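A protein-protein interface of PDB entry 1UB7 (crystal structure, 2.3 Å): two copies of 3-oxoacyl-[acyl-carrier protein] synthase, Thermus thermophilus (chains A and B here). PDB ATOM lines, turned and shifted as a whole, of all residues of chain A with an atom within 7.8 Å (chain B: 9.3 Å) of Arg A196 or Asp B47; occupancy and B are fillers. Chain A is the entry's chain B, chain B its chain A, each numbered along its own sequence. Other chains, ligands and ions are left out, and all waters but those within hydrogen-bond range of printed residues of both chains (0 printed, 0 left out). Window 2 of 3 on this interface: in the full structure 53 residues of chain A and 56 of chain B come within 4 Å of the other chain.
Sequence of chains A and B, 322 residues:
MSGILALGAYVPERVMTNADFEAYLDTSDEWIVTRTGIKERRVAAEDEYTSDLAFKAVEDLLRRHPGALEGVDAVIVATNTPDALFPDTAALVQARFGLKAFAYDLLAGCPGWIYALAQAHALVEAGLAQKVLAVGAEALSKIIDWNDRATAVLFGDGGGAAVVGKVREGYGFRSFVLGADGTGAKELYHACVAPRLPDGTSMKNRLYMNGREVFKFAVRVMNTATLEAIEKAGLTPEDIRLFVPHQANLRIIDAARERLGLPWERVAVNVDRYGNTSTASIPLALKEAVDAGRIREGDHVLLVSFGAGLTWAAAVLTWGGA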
ATOM      1  N   ALA A 191       5.430 -24.897  -7.547  1.00  0.00           N
ATOM      2  CA  ALA A 191       6.535 -24.532  -8.431  1.00  0.00           C
ATOM      3  C   ALA A 191       6.667 -23.032  -8.682  1.00  0.00           C
ATOM      4  O   ALA A 191       5.707 -22.276  -8.530  1.00  0.00           O
ATOM      5  CB  ALA A 191       6.391 -25.277  -9.760  1.00  0.00           C
ATOM      6  N   VAL A 193       9.980 -21.866 -10.776  1.00  0.00           N
ATOM      7  CA  VAL A 193      10.834 -21.808 -11.955  1.00  0.00           C
ATOM      8  C   VAL A 193      11.045 -23.201 -12.559  1.00  0.00           C
ATOM      9  O   VAL A 193      11.334 -23.332 -13.753  1.00  0.00           O
ATOM     10  CB  VAL A 193      12.200 -21.169 -11.606  1.00  0.00           C
ATOM     11  CG1 VAL A 193      13.081 -21.110 -12.835  1.00  0.00           C
ATOM     12  CG2 VAL A 193      11.991 -19.771 -11.065  1.00  0.00           C
ATOM     13  N   ALA A 194      10.877 -24.236 -11.738  1.00  0.00           N
ATOM     14  CA  ALA A 194      11.053 -25.619 -12.189  1.00  0.00           C
ATOM     15  C   ALA A 194       9.738 -26.417 -12.235  1.00  0.00           C
ATOM     16  O   ALA A 194       8.826 -26.180 -11.437  1.00  0.00           O
ATOM     17  CB  ALA A 194      12.059 -26.324 -11.286  1.00  0.00           C
ATOM     18  N   PRO A 195       9.621 -27.370 -13.183  1.00  0.00           N
ATOM     19  CA  PRO A 195       8.411 -28.188 -13.307  1.00  0.00           C
ATOM     20  C   PRO A 195       8.525 -29.506 -12.545  1.00  0.00           C
ATOM     21  O   PRO A 195       7.605 -30.322 -12.565  1.00  0.00           O
ATOM     22  CB  PRO A 195       8.312 -28.405 -14.809  1.00  0.00           C
ATOM     23  CG  PRO A 195       9.737 -28.613 -15.170  1.00  0.00           C
ATOM     24  CD  PRO A 195      10.461 -27.519 -14.386  1.00  0.00           C
ATOM     25  N   ARG A 196       9.657 -29.714 -11.881  1.00  0.00           N
ATOM     26  CA  ARG A 196       9.874 -30.940 -11.126  1.00  0.00           C
ATOM     27  C   ARG A 196      10.772 -30.749  -9.901  1.00  0.00           C
ATOM     28  O   ARG A 196      11.637 -29.867  -9.868  1.00  0.00           O
ATOM     29  CB  ARG A 196      10.458 -32.018 -12.048  1.00  0.00           C
ATOM     30  CG  ARG A 196      11.725 -31.599 -12.786  1.00  0.00           C
ATOM     31  CD  ARG A 196      12.890 -31.424 -11.825  1.00  0.00           C
ATOM     32  NE  ARG A 196      14.135 -31.050 -12.490  1.00  0.00           N
ATOM     33  CZ  ARG A 196      15.253 -30.720 -11.847  1.00  0.00           C
ATOM     34  NH1 ARG A 196      15.286 -30.711 -10.516  1.00  0.00           N
ATOM     35  NH2 ARG A 196      16.341 -30.411 -12.534  1.00  0.00           N
ATOM     36  N   LEU A 197      10.553 -31.581  -8.889  1.00  0.00           N
ATOM     37  CA  LEU A 197      11.343 -31.522  -7.668  1.00  0.00           C
ATOM     38  C   LEU A 197      12.524 -32.481  -7.812  1.00  0.00           C
ATOM     39  O   LEU A 197      12.477 -33.414  -8.618  1.00  0.00           O
ATOM     40  CB  LEU A 197      10.473 -31.902  -6.460  1.00  0.00           C
ATOM     41  CG  LEU A 197       9.406 -30.861  -6.098  1.00  0.00           C
ATOM     42  CD1 LEU A 197       8.369 -31.473  -5.179  1.00  0.00           C
ATOM     43  CD2 LEU A 197      10.069 -29.654  -5.446  1.00  0.00           C
ATOM     44  N   PRO A 198      13.610 -32.246  -7.053  1.00  0.00           N
ATOM     45  CA  PRO A 198      14.798 -33.096  -7.107  1.00  0.00           C
ATOM     46  C   PRO A 198      14.511 -34.594  -7.125  1.00  0.00           C
ATOM     47  O   PRO A 198      15.076 -35.316  -7.946  1.00  0.00           O
ATOM     48  CB  PRO A 198      15.579 -32.656  -5.877  1.00  0.00           C
ATOM     49  CG  PRO A 198      15.348 -31.195  -5.895  1.00  0.00           C
ATOM     50  CD  PRO A 198      13.847 -31.102  -6.154  1.00  0.00           C
ATOM     51  N   ASP A 199      13.633 -35.064  -6.242  1.00  0.00           N
ATOM     52  CA  ASP A 199      13.322 -36.493  -6.202  1.00  0.00           C
ATOM     53  C   ASP A 199      12.527 -36.958  -7.430  1.00  0.00           C
ATOM     54  O   ASP A 199      12.183 -38.135  -7.553  1.00  0.00           O
ATOM     55  CB  ASP A 199      12.573 -36.844  -4.906  1.00  0.00           C
ATOM     56  CG  ASP A 199      11.112 -36.454  -4.943  1.00  0.00           C
ATOM     57  OD1 ASP A 199      10.778 -35.388  -5.503  1.00  0.00           O
ATOM     58  OD2 ASP A 199      10.296 -37.217  -4.394  1.00  0.00           O
ATOM     59  N   GLY A 200      12.247 -36.029  -8.342  1.00  0.00           N
ATOM     60  CA  GLY A 200      11.517 -36.374  -9.547  1.00  0.00           C
ATOM     61  C   GLY A 200      10.022 -36.103  -9.523  1.00  0.00           C
ATOM     62  O   GLY A 200       9.355 -36.232 -10.551  1.00  0.00           O
ATOM     63  N   THR A 201       9.490 -35.733  -8.363  1.00  0.00           N
ATOM     64  CA  THR A 201       8.064 -35.454  -8.237  1.00  0.00           C
ATOM     65  C   THR A 201       7.616 -34.321  -9.155  1.00  0.00           C
ATOM     66  O   THR A 201       7.935 -33.155  -8.921  1.00  0.00           O
ATOM     67  CB  THR A 201       7.689 -35.080  -6.787  1.00  0.00           C
ATOM     68  OG1 THR A 201       7.803 -36.236  -5.947  1.00  0.00           O
ATOM     69  CG2 THR A 201       6.265 -34.535  -6.723  1.00  0.00           C
ATOM     70  N   SER A 202       6.873 -34.668 -10.202  1.00  0.00           N
ATOM     71  CA  SER A 202       6.372 -33.671 -11.137  1.00  0.00           C
ATOM     72  C   SER A 202       5.438 -32.729 -10.386  1.00  0.00           C
ATOM     73  O   SER A 202       4.600 -33.172  -9.601  1.00  0.00           O
ATOM     74  CB  SER A 202       5.611 -34.347 -12.282  1.00  0.00           C
ATOM     75  OG  SER A 202       5.060 -33.387 -13.172  1.00  0.00           O
ATOM     76  N   MET A 203       5.589 -31.430 -10.621  1.00  0.00           N
ATOM     77  CA  MET A 203       4.748 -30.438  -9.961  1.00  0.00           C
ATOM     78  C   MET A 203       3.648 -29.936 -10.888  1.00  0.00           C
ATOM     79  O   MET A 203       3.907 -29.603 -12.047  1.00  0.00           O
ATOM     80  CB  MET A 203       5.587 -29.239  -9.491  1.00  0.00           C
ATOM     81  CG  MET A 203       6.559 -29.533  -8.359  1.00  0.00           C
ATOM     82  SD  MET A 203       7.355 -28.026  -7.750  1.00  0.00           S
ATOM     83  CE  MET A 203       8.886 -28.021  -8.698  1.00  0.00           C
ATOM     84  N   LYS A 204       2.418 -29.897 -10.380  1.00  0.00           N
ATOM     85  CA  LYS A 204       1.290 -29.396 -11.160  1.00  0.00           C
ATOM     86  C   LYS A 204       1.465 -27.878 -11.244  1.00  0.00           C
ATOM     87  O   LYS A 204       2.329 -27.317 -10.567  1.00  0.00           O
ATOM     88  CB  LYS A 204      -0.043 -29.727 -10.476  1.00  0.00           C
ATOM     89  CG  LYS A 204      -0.448 -31.198 -10.503  1.00  0.00           C
ATOM     90  CD  LYS A 204       0.452 -32.060  -9.634  1.00  0.00           C
ATOM     91  CE  LYS A 204      -0.095 -33.478  -9.512  1.00  0.00           C
ATOM     92  NZ  LYS A 204      -0.193 -34.174 -10.827  1.00  0.00           N
ATOM     93  N   VAL B  43      24.980 -21.586 -19.724  1.00  0.00           N
ATOM     94  CA  VAL B  43      23.525 -21.752 -19.660  1.00  0.00           C
ATOM     95  C   VAL B  43      23.165 -23.154 -19.155  1.00  0.00           C
ATOM     96  O   VAL B  43      23.678 -24.161 -19.658  1.00  0.00           O
ATOM     97  CB  VAL B  43      22.871 -21.522 -21.052  1.00  0.00           C
ATOM     98  CG1 VAL B  43      21.352 -21.636 -20.955  1.00  0.00           C
ATOM     99  CG2 VAL B  43      23.264 -20.144 -21.588  1.00  0.00           C
ATOM    100  N   ALA B  44      22.278 -23.208 -18.162  1.00  0.00           N
ATOM    101  CA  ALA B  44      21.866 -24.477 -17.565  1.00  0.00           C
ATOM    102  C   ALA B  44      21.200 -25.410 -18.562  1.00  0.00           C
ATOM    103  O   ALA B  44      20.442 -24.969 -19.429  1.00  0.00           O
ATOM    104  CB  ALA B  44      20.921 -24.218 -16.389  1.00  0.00           C
ATOM    105  N   ALA B  45      21.476 -26.705 -18.435  1.00  0.00           N
ATOM    106  CA  ALA B  45      20.873 -27.675 -19.335  1.00  0.00           C
ATOM    107  C   ALA B  45      19.350 -27.557 -19.231  1.00  0.00           C
ATOM    108  O   ALA B  45      18.822 -26.974 -18.277  1.00  0.00           O
ATOM    109  CB  ALA B  45      21.327 -29.078 -18.981  1.00  0.00           C
ATOM    110  N   GLU B  46      18.650 -28.117 -20.211  1.00  0.00           N
ATOM    111  CA  GLU B  46      17.196 -28.045 -20.264  1.00  0.00           C
ATOM    112  C   GLU B  46      16.497 -28.404 -18.956  1.00  0.00           C
ATOM    113  O   GLU B  46      15.582 -27.704 -18.520  1.00  0.00           O
ATOM    114  CB  GLU B  46      16.674 -28.953 -21.373  1.00  0.00           C
ATOM    115  CG  GLU B  46      15.213 -28.708 -21.727  1.00  0.00           C
ATOM    116  CD  GLU B  46      14.608 -29.848 -22.530  1.00  0.00           C
ATOM    117  OE1 GLU B  46      15.256 -30.301 -23.500  1.00  0.00           O
ATOM    118  OE2 GLU B  46      13.484 -30.286 -22.190  1.00  0.00           O
ATOM    119  N   ASP B  47      16.917 -29.499 -18.338  1.00  0.00           N
ATOM    120  CA  ASP B  47      16.308 -29.940 -17.096  1.00  0.00           C
ATOM    121  C   ASP B  47      17.249 -29.711 -15.911  1.00  0.00           C
ATOM    122  O   ASP B  47      17.307 -30.522 -14.983  1.00  0.00           O
ATOM    123  CB  ASP B  47      15.969 -31.417 -17.215  1.00  0.00           C
ATOM    124  CG  ASP B  47      17.200 -32.264 -17.486  1.00  0.00           C
ATOM    125  OD1 ASP B  47      18.197 -31.714 -18.009  1.00  0.00           O
ATOM    126  OD2 ASP B  47      17.178 -33.477 -17.184  1.00  0.00           O
ATOM    127  N   GLU B  48      17.995 -28.612 -15.947  1.00  0.00           N
ATOM    128  CA  GLU B  48      18.916 -28.291 -14.864  1.00  0.00           C
ATOM    129  C   GLU B  48      18.446 -26.992 -14.231  1.00  0.00           C
ATOM    130  O   GLU B  48      18.493 -25.946 -14.868  1.00  0.00           O
ATOM    131  CB  GLU B  48      20.330 -28.127 -15.417  1.00  0.00           C
ATOM    132  CG  GLU B  48      21.374 -27.727 -14.398  1.00  0.00           C
ATOM    133  CD  GLU B  48      22.773 -27.617 -15.004  1.00  0.00           C
ATOM    134  OE1 GLU B  48      22.885 -27.097 -16.134  1.00  0.00           O
ATOM    135  OE2 GLU B  48      23.759 -28.032 -14.350  1.00  0.00           O
ATOM    136  N   TYR B  49      17.989 -27.049 -12.981  1.00  0.00           N
ATOM    137  CA  TYR B  49      17.494 -25.845 -12.309  1.00  0.00           C
ATOM    138  C   TYR B  49      18.348 -25.298 -11.181  1.00  0.00           C
ATOM    139  O   TYR B  49      19.405 -25.847 -10.856  1.00  0.00           O
ATOM    140  CB  TYR B  49      16.074 -26.077 -11.816  1.00  0.00           C
ATOM    141  CG  TYR B  49      15.129 -26.308 -12.962  1.00  0.00           C
ATOM    142  CD1 TYR B  49      14.982 -27.575 -13.530  1.00  0.00           C
ATOM    143  CD2 TYR B  49      14.442 -25.242 -13.540  1.00  0.00           C
ATOM    144  CE1 TYR B  49      14.175 -27.775 -14.649  1.00  0.00           C
ATOM    145  CE2 TYR B  49      13.635 -25.430 -14.660  1.00  0.00           C
ATOM    146  CZ  TYR B  49      13.506 -26.696 -15.207  1.00  0.00           C
ATOM    147  OH  TYR B  49      12.702 -26.875 -16.308  1.00  0.00           O
ATOM    148  N   THR B  50      17.885 -24.204 -10.584  1.00  0.00           N
ATOM    149  CA  THR B  50      18.634 -23.567  -9.501  1.00  0.00           C
ATOM    150  C   THR B  50      19.121 -24.522  -8.412  1.00  0.00           C
ATOM    151  O   THR B  50      20.261 -24.406  -7.949  1.00  0.00           O
ATOM    152  CB  THR B  50      17.827 -22.444  -8.853  1.00  0.00           C
ATOM    153  OG1 THR B  50      17.713 -21.359  -9.782  1.00  0.00           O
ATOM    154  CG2 THR B  50      18.513 -21.965  -7.569  1.00  0.00           C
ATOM    155  N   SER B  51      18.270 -25.465  -8.017  1.00  0.00           N
ATOM    156  CA  SER B  51      18.655 -26.433  -7.001  1.00  0.00           C
ATOM    157  C   SER B  51      19.819 -27.290  -7.506  1.00  0.00           C
ATOM    158  O   SER B  51      20.737 -27.628  -6.745  1.00  0.00           O
ATOM    159  CB  SER B  51      17.456 -27.314  -6.624  1.00  0.00           C
ATOM    160  OG  SER B  51      16.880 -27.904  -7.765  1.00  0.00           O
ATOM    161  N   ASP B  52      19.799 -27.618  -8.793  1.00  0.00           N
ATOM    162  CA  ASP B  52      20.876 -28.429  -9.370  1.00  0.00           C
ATOM    163  C   ASP B  52      22.175 -27.645  -9.367  1.00  0.00           C
ATOM    164  O   ASP B  52      23.238 -28.184  -9.046  1.00  0.00           O
ATOM    165  CB  ASP B  52      20.532 -28.839 -10.794  1.00  0.00           C
ATOM    166  CG  ASP B  52      19.229 -29.579 -10.868  1.00  0.00           C
ATOM    167  OD1 ASP B  52      19.178 -30.734 -10.385  1.00  0.00           O
ATOM    168  OD2 ASP B  52      18.257 -28.995 -11.392  1.00  0.00           O
ATOM    169  N   LEU B  53      22.090 -26.371  -9.731  1.00  0.00           N
ATOM    170  CA  LEU B  53      23.279 -25.554  -9.737  1.00  0.00           C
ATOM    171  C   LEU B  53      23.788 -25.507  -8.299  1.00  0.00           C
ATOM    172  O   LEU B  53      24.995 -25.567  -8.066  1.00  0.00           O
ATOM    173  CB  LEU B  53      22.963 -24.147 -10.242  1.00  0.00           C
ATOM    174  CG  LEU B  53      22.232 -24.040 -11.588  1.00  0.00           C
ATOM    175  CD1 LEU B  53      22.015 -22.563 -11.926  1.00  0.00           C
ATOM    176  CD2 LEU B  53      23.044 -24.729 -12.686  1.00  0.00           C
ATOM    177  N   PHE B  55      23.301 -27.823  -5.918  1.00  0.00           N
ATOM    178  CA  PHE B  55      23.867 -29.124  -5.565  1.00  0.00           C
ATOM    179  C   PHE B  55      25.286 -29.226  -6.118  1.00  0.00           C
ATOM    180  O   PHE B  55      26.224 -29.580  -5.398  1.00  0.00           O
ATOM    181  CB  PHE B  55      23.035 -30.289  -6.130  1.00  0.00           C
ATOM    182  CG  PHE B  55      21.608 -30.353  -5.625  1.00  0.00           C
ATOM    183  CD1 PHE B  55      21.220 -29.702  -4.447  1.00  0.00           C
ATOM    184  CD2 PHE B  55      20.646 -31.078  -6.338  1.00  0.00           C
ATOM    185  CE1 PHE B  55      19.892 -29.768  -3.995  1.00  0.00           C
ATOM    186  CE2 PHE B  55      19.320 -31.150  -5.894  1.00  0.00           C
ATOM    187  CZ  PHE B  55      18.946 -30.489  -4.718  1.00  0.00           C
ATOM    188  N   LYS B  56      25.440 -28.905  -7.401  1.00  0.00           N
ATOM    189  CA  LYS B  56      26.744 -28.968  -8.046  1.00  0.00           C
ATOM    190  C   LYS B  56      27.786 -28.055  -7.410  1.00  0.00           C
ATOM    191  O   LYS B  56      28.962 -28.408  -7.339  1.00  0.00           O
ATOM    192  CB  LYS B  56      26.610 -28.683  -9.549  1.00  0.00           C
ATOM    193  CG  LYS B  56      26.285 -29.943 -10.349  1.00  0.00           C
ATOM    194  CD  LYS B  56      25.225 -29.700 -11.396  1.00  0.00           C
ATOM    195  CE  LYS B  56      24.693 -31.013 -11.975  1.00  0.00           C
ATOM    196  NZ  LYS B  56      23.570 -30.754 -12.939  1.00  0.00           N
ATOM    197  N   PRO B  82      14.245 -19.426  -7.317  1.00  0.00           N
ATOM    198  CA  PRO B  82      14.083 -20.740  -6.685  1.00  0.00           C
ATOM    199  C   PRO B  82      13.180 -21.673  -7.507  1.00  0.00           C
ATOM    200  O   PRO B  82      12.291 -21.217  -8.238  1.00  0.00           O
ATOM    201  CB  PRO B  82      13.487 -20.391  -5.326  1.00  0.00           C
ATOM    202  CG  PRO B  82      12.610 -19.220  -5.663  1.00  0.00           C
ATOM    203  CD  PRO B  82      13.494 -18.394  -6.575  1.00  0.00           C
ATOM    204  N   ASP B  83      13.427 -22.975  -7.402  1.00  0.00           N
ATOM    205  CA  ASP B  83      12.626 -23.957  -8.119  1.00  0.00           C
ATOM    206  C   ASP B  83      11.143 -23.764  -7.855  1.00  0.00           C
ATOM    207  O   ASP B  83      10.336 -23.794  -8.781  1.00  0.00           O
ATOM    208  CB  ASP B  83      13.028 -25.373  -7.706  1.00  0.00           C
ATOM    209  CG  ASP B  83      14.409 -25.746  -8.187  1.00  0.00           C
ATOM    210  OD1 ASP B  83      15.236 -24.836  -8.410  1.00  0.00           O
ATOM    211  OD2 ASP B  83      14.670 -26.956  -8.331  1.00  0.00           O
ATOM    212  N   ALA B  84      10.779 -23.575  -6.589  1.00  0.00           N
ATOM    213  CA  ALA B  84       9.380 -23.376  -6.226  1.00  0.00           C
ATOM    214  C   ALA B  84       9.233 -22.315  -5.138  1.00  0.00           C
ATOM    215  O   ALA B  84      10.225 -21.929  -4.514  1.00  0.00           O
ATOM    216  CB  ALA B  84       8.793 -24.688  -5.744  1.00  0.00           C
ATOM    217  N   PRO B  87       8.524 -26.199  -1.731  1.00  0.00           N
ATOM    218  CA  PRO B  87       9.538 -26.057  -0.682  1.00  0.00           C
ATOM    219  C   PRO B  87      10.665 -25.116  -1.124  1.00  0.00           C
ATOM    220  O   PRO B  87      10.845 -24.874  -2.319  1.00  0.00           O
ATOM    221  CB  PRO B  87      10.022 -27.493  -0.495  1.00  0.00           C
ATOM    222  CG  PRO B  87       9.978 -28.020  -1.911  1.00  0.00           C
ATOM    223  CD  PRO B  87       8.645 -27.502  -2.410  1.00  0.00           C
ATOM    224  N   THR B  89      14.549 -23.913  -1.800  1.00  0.00           N
ATOM    225  CA  THR B  89      15.694 -24.586  -2.359  1.00  0.00           C
ATOM    226  C   THR B  89      16.683 -24.999  -1.271  1.00  0.00           C
ATOM    227  O   THR B  89      17.392 -25.984  -1.439  1.00  0.00           O
ATOM    228  CB  THR B  89      16.370 -23.664  -3.397  1.00  0.00           C
ATOM    229  OG1 THR B  89      15.367 -23.184  -4.291  1.00  0.00           O
ATOM    230  CG2 THR B  89      17.425 -24.403  -4.188  1.00  0.00           C
ATOM    231  N   LEU B  92      15.918 -28.388  -0.112  1.00  0.00           N
ATOM    232  CA  LEU B  92      16.322 -29.409  -1.078  1.00  0.00           C
ATOM    233  C   LEU B  92      17.819 -29.699  -0.931  1.00  0.00           C
ATOM    234  O   LEU B  92      18.256 -30.849  -1.044  1.00  0.00           O
ATOM    235  CB  LEU B  92      16.013 -28.950  -2.514  1.00  0.00           C
ATOM    236  CG  LEU B  92      14.565 -28.523  -2.810  1.00  0.00           C
ATOM    237  CD1 LEU B  92      14.428 -28.043  -4.258  1.00  0.00           C
ATOM    238  CD2 LEU B  92      13.636 -29.689  -2.554  1.00  0.00           C
ATOM    239  N   ALA B 139      19.445 -19.338 -11.813  1.00  0.00           N
ATOM    240  CA  ALA B 139      19.194 -19.911 -13.134  1.00  0.00           C
ATOM    241  C   ALA B 139      18.399 -18.835 -13.875  1.00  0.00           C
ATOM    242  O   ALA B 139      17.217 -19.000 -14.155  1.00  0.00           O
ATOM    243  CB  ALA B 139      18.371 -21.188 -13.021  1.00  0.00           C
ATOM    244  N   SER B 141      18.516 -17.934 -16.871  1.00  0.00           N
ATOM    245  CA  SER B 141      18.097 -18.351 -18.200  1.00  0.00           C
ATOM    246  C   SER B 141      16.688 -18.918 -18.193  1.00  0.00           C
ATOM    247  O   SER B 141      16.168 -19.296 -19.233  1.00  0.00           O
ATOM    248  CB  SER B 141      19.060 -19.401 -18.757  1.00  0.00           C
ATOM    249  OG  SER B 141      18.961 -20.613 -18.045  1.00  0.00           O
ATOM    250  N   LYS B 142      16.062 -18.965 -17.027  1.00  0.00           N
ATOM    251  CA  LYS B 142      14.715 -19.523 -16.941  1.00  0.00           C
ATOM    252  C   LYS B 142      13.626 -18.460 -16.862  1.00  0.00           C
ATOM    253  O   LYS B 142      12.449 -18.775 -17.017  1.00  0.00           O
ATOM    254  CB  LYS B 142      14.600 -20.442 -15.720  1.00  0.00           C
ATOM    255  CG  LYS B 142      15.752 -21.420 -15.549  1.00  0.00           C
ATOM    256  CD  LYS B 142      15.713 -22.564 -16.532  1.00  0.00           C
ATOM    257  CE  LYS B 142      16.830 -23.558 -16.231  1.00  0.00           C
ATOM    258  NZ  LYS B 142      16.694 -24.828 -16.997  1.00  0.00           N
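OD2 of Asp B52 is in salt-bridge range of NH2 of Arg A196 (2.6 Å).
The backbone carbonyl oxygen of Asp B83 is in hydrogen-bond range of the backbone NH of Val A193, 2.8 Å away.
O of Asp B83 sits at hydrogen-bond distance from N of Ala A194 (3.0 Å).
The backbone carbonyl oxygen (O) of Pro B82 sits close to the backbone NH (N) of Val A193 (3.5 Å).
The backbone carbonyl oxygen of Asp B47 is in hydrogen-bond range of the guanidinium group of Arg A196.
SD of Met A203 lies close to N of Ala A191, 3.7 Å away.
The side-chain amino group (NZ) of Lys B142 lies within hydrogen-bond range of the backbone carbonyl oxygen (O) of Glu B46 (3.4 Å).
The backbone carbonyl oxygen (O) of Pro A195 is in hydrogen-bond range of the backbone NH (N) of Met A203, at 3.0 Å.
The side-chain amino group (NZ) of Lys B142 is in hydrogen-bond range of the backbone carbonyl oxygen (O) of Glu B48.
N of Tyr B49 lies within hydrogen-bond range of OD2 of Asp B52 (2.5 Å).
N of Thr B50 sits at hydrogen-bond distance from OD1 of Asp B83 (3.5 Å).
C of Ala A191 touches O of Asp B83, at 3.7 Å.
Ala B84 touches Ala A191 (CB to CA, 3.5 Å).
O of Val A193 touches CE2 of Tyr B49, at 3.2 Å.
Val A193 touches Lys B142.
Ala A194 touches Tyr B49 (CB to CD2, 3.5 Å).
Pro A195 touches Tyr B49 (CD to OH, 3.0 Å).
Arg A196 touches Tyr B49 (NH2 to CD1, 3.3 Å).
Pro B87 touches Leu A197 (CG to CD2, 3.9 Å).
CZ of Phe B55 touches CG of Pro A198 (3.9 Å).
Pro A198 touches Leu B92.
Of the printed residues of chain B, Ala A191 touches Asp B83 (3.7 Å) and Ala B84 (3.5 Å).
Of the printed residues of chain B, Val A193 touches Tyr B49, Pro B82, Asp B83 and Lys B142.
Pro A195 touches just one residue of chain B: Tyr B49.
Of the printed residues of chain B, Arg A196 touches Asp B47, Tyr B49 and Asp B52.
Printed residues of chain B within 4 Å of Pro A198: Phe B55 and Leu B92.
Val B43 touches none of the printed residues of chain A.
Of the printed residues of chain A, Asp B52 touches Arg A196 (2.6 Å).
Lys B56 touches none of the printed residues of chain A.
Of the printed residues of chain A, Lys B142 touches Val A193 (3.3 Å).
The nearest residue of chain B that does not touch Arg A196 is Glu B48 (4.1 Å).
The nearest printed residue of chain A that does not touch Asp B52 is Pro A198 (5.9 Å).
Of the 13 printed residues of chain A, 7 touch a printed residue of chain B.
Hydrophobic or aromatic side chains of chain A that line the printed part of chain B: Val A193, Ala A194, Pro A195, Leu A197 and Pro A198.
Hydrophobic or aromatic side chains of chain B within 4 Å of the printed part of chain A: Tyr B49, Phe B55, Ala B84, Pro B87 and Leu B92.
Along chain B the printed residues that touch a printed residue of chain A span positions 47 to 142.
Among the printed residues, 15 pairs touch across the chains.
No position is printed for both chains.
Of the 15 pairs that touch across the chains among the printed residues, none has its exchanged pair printed and touching as well.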
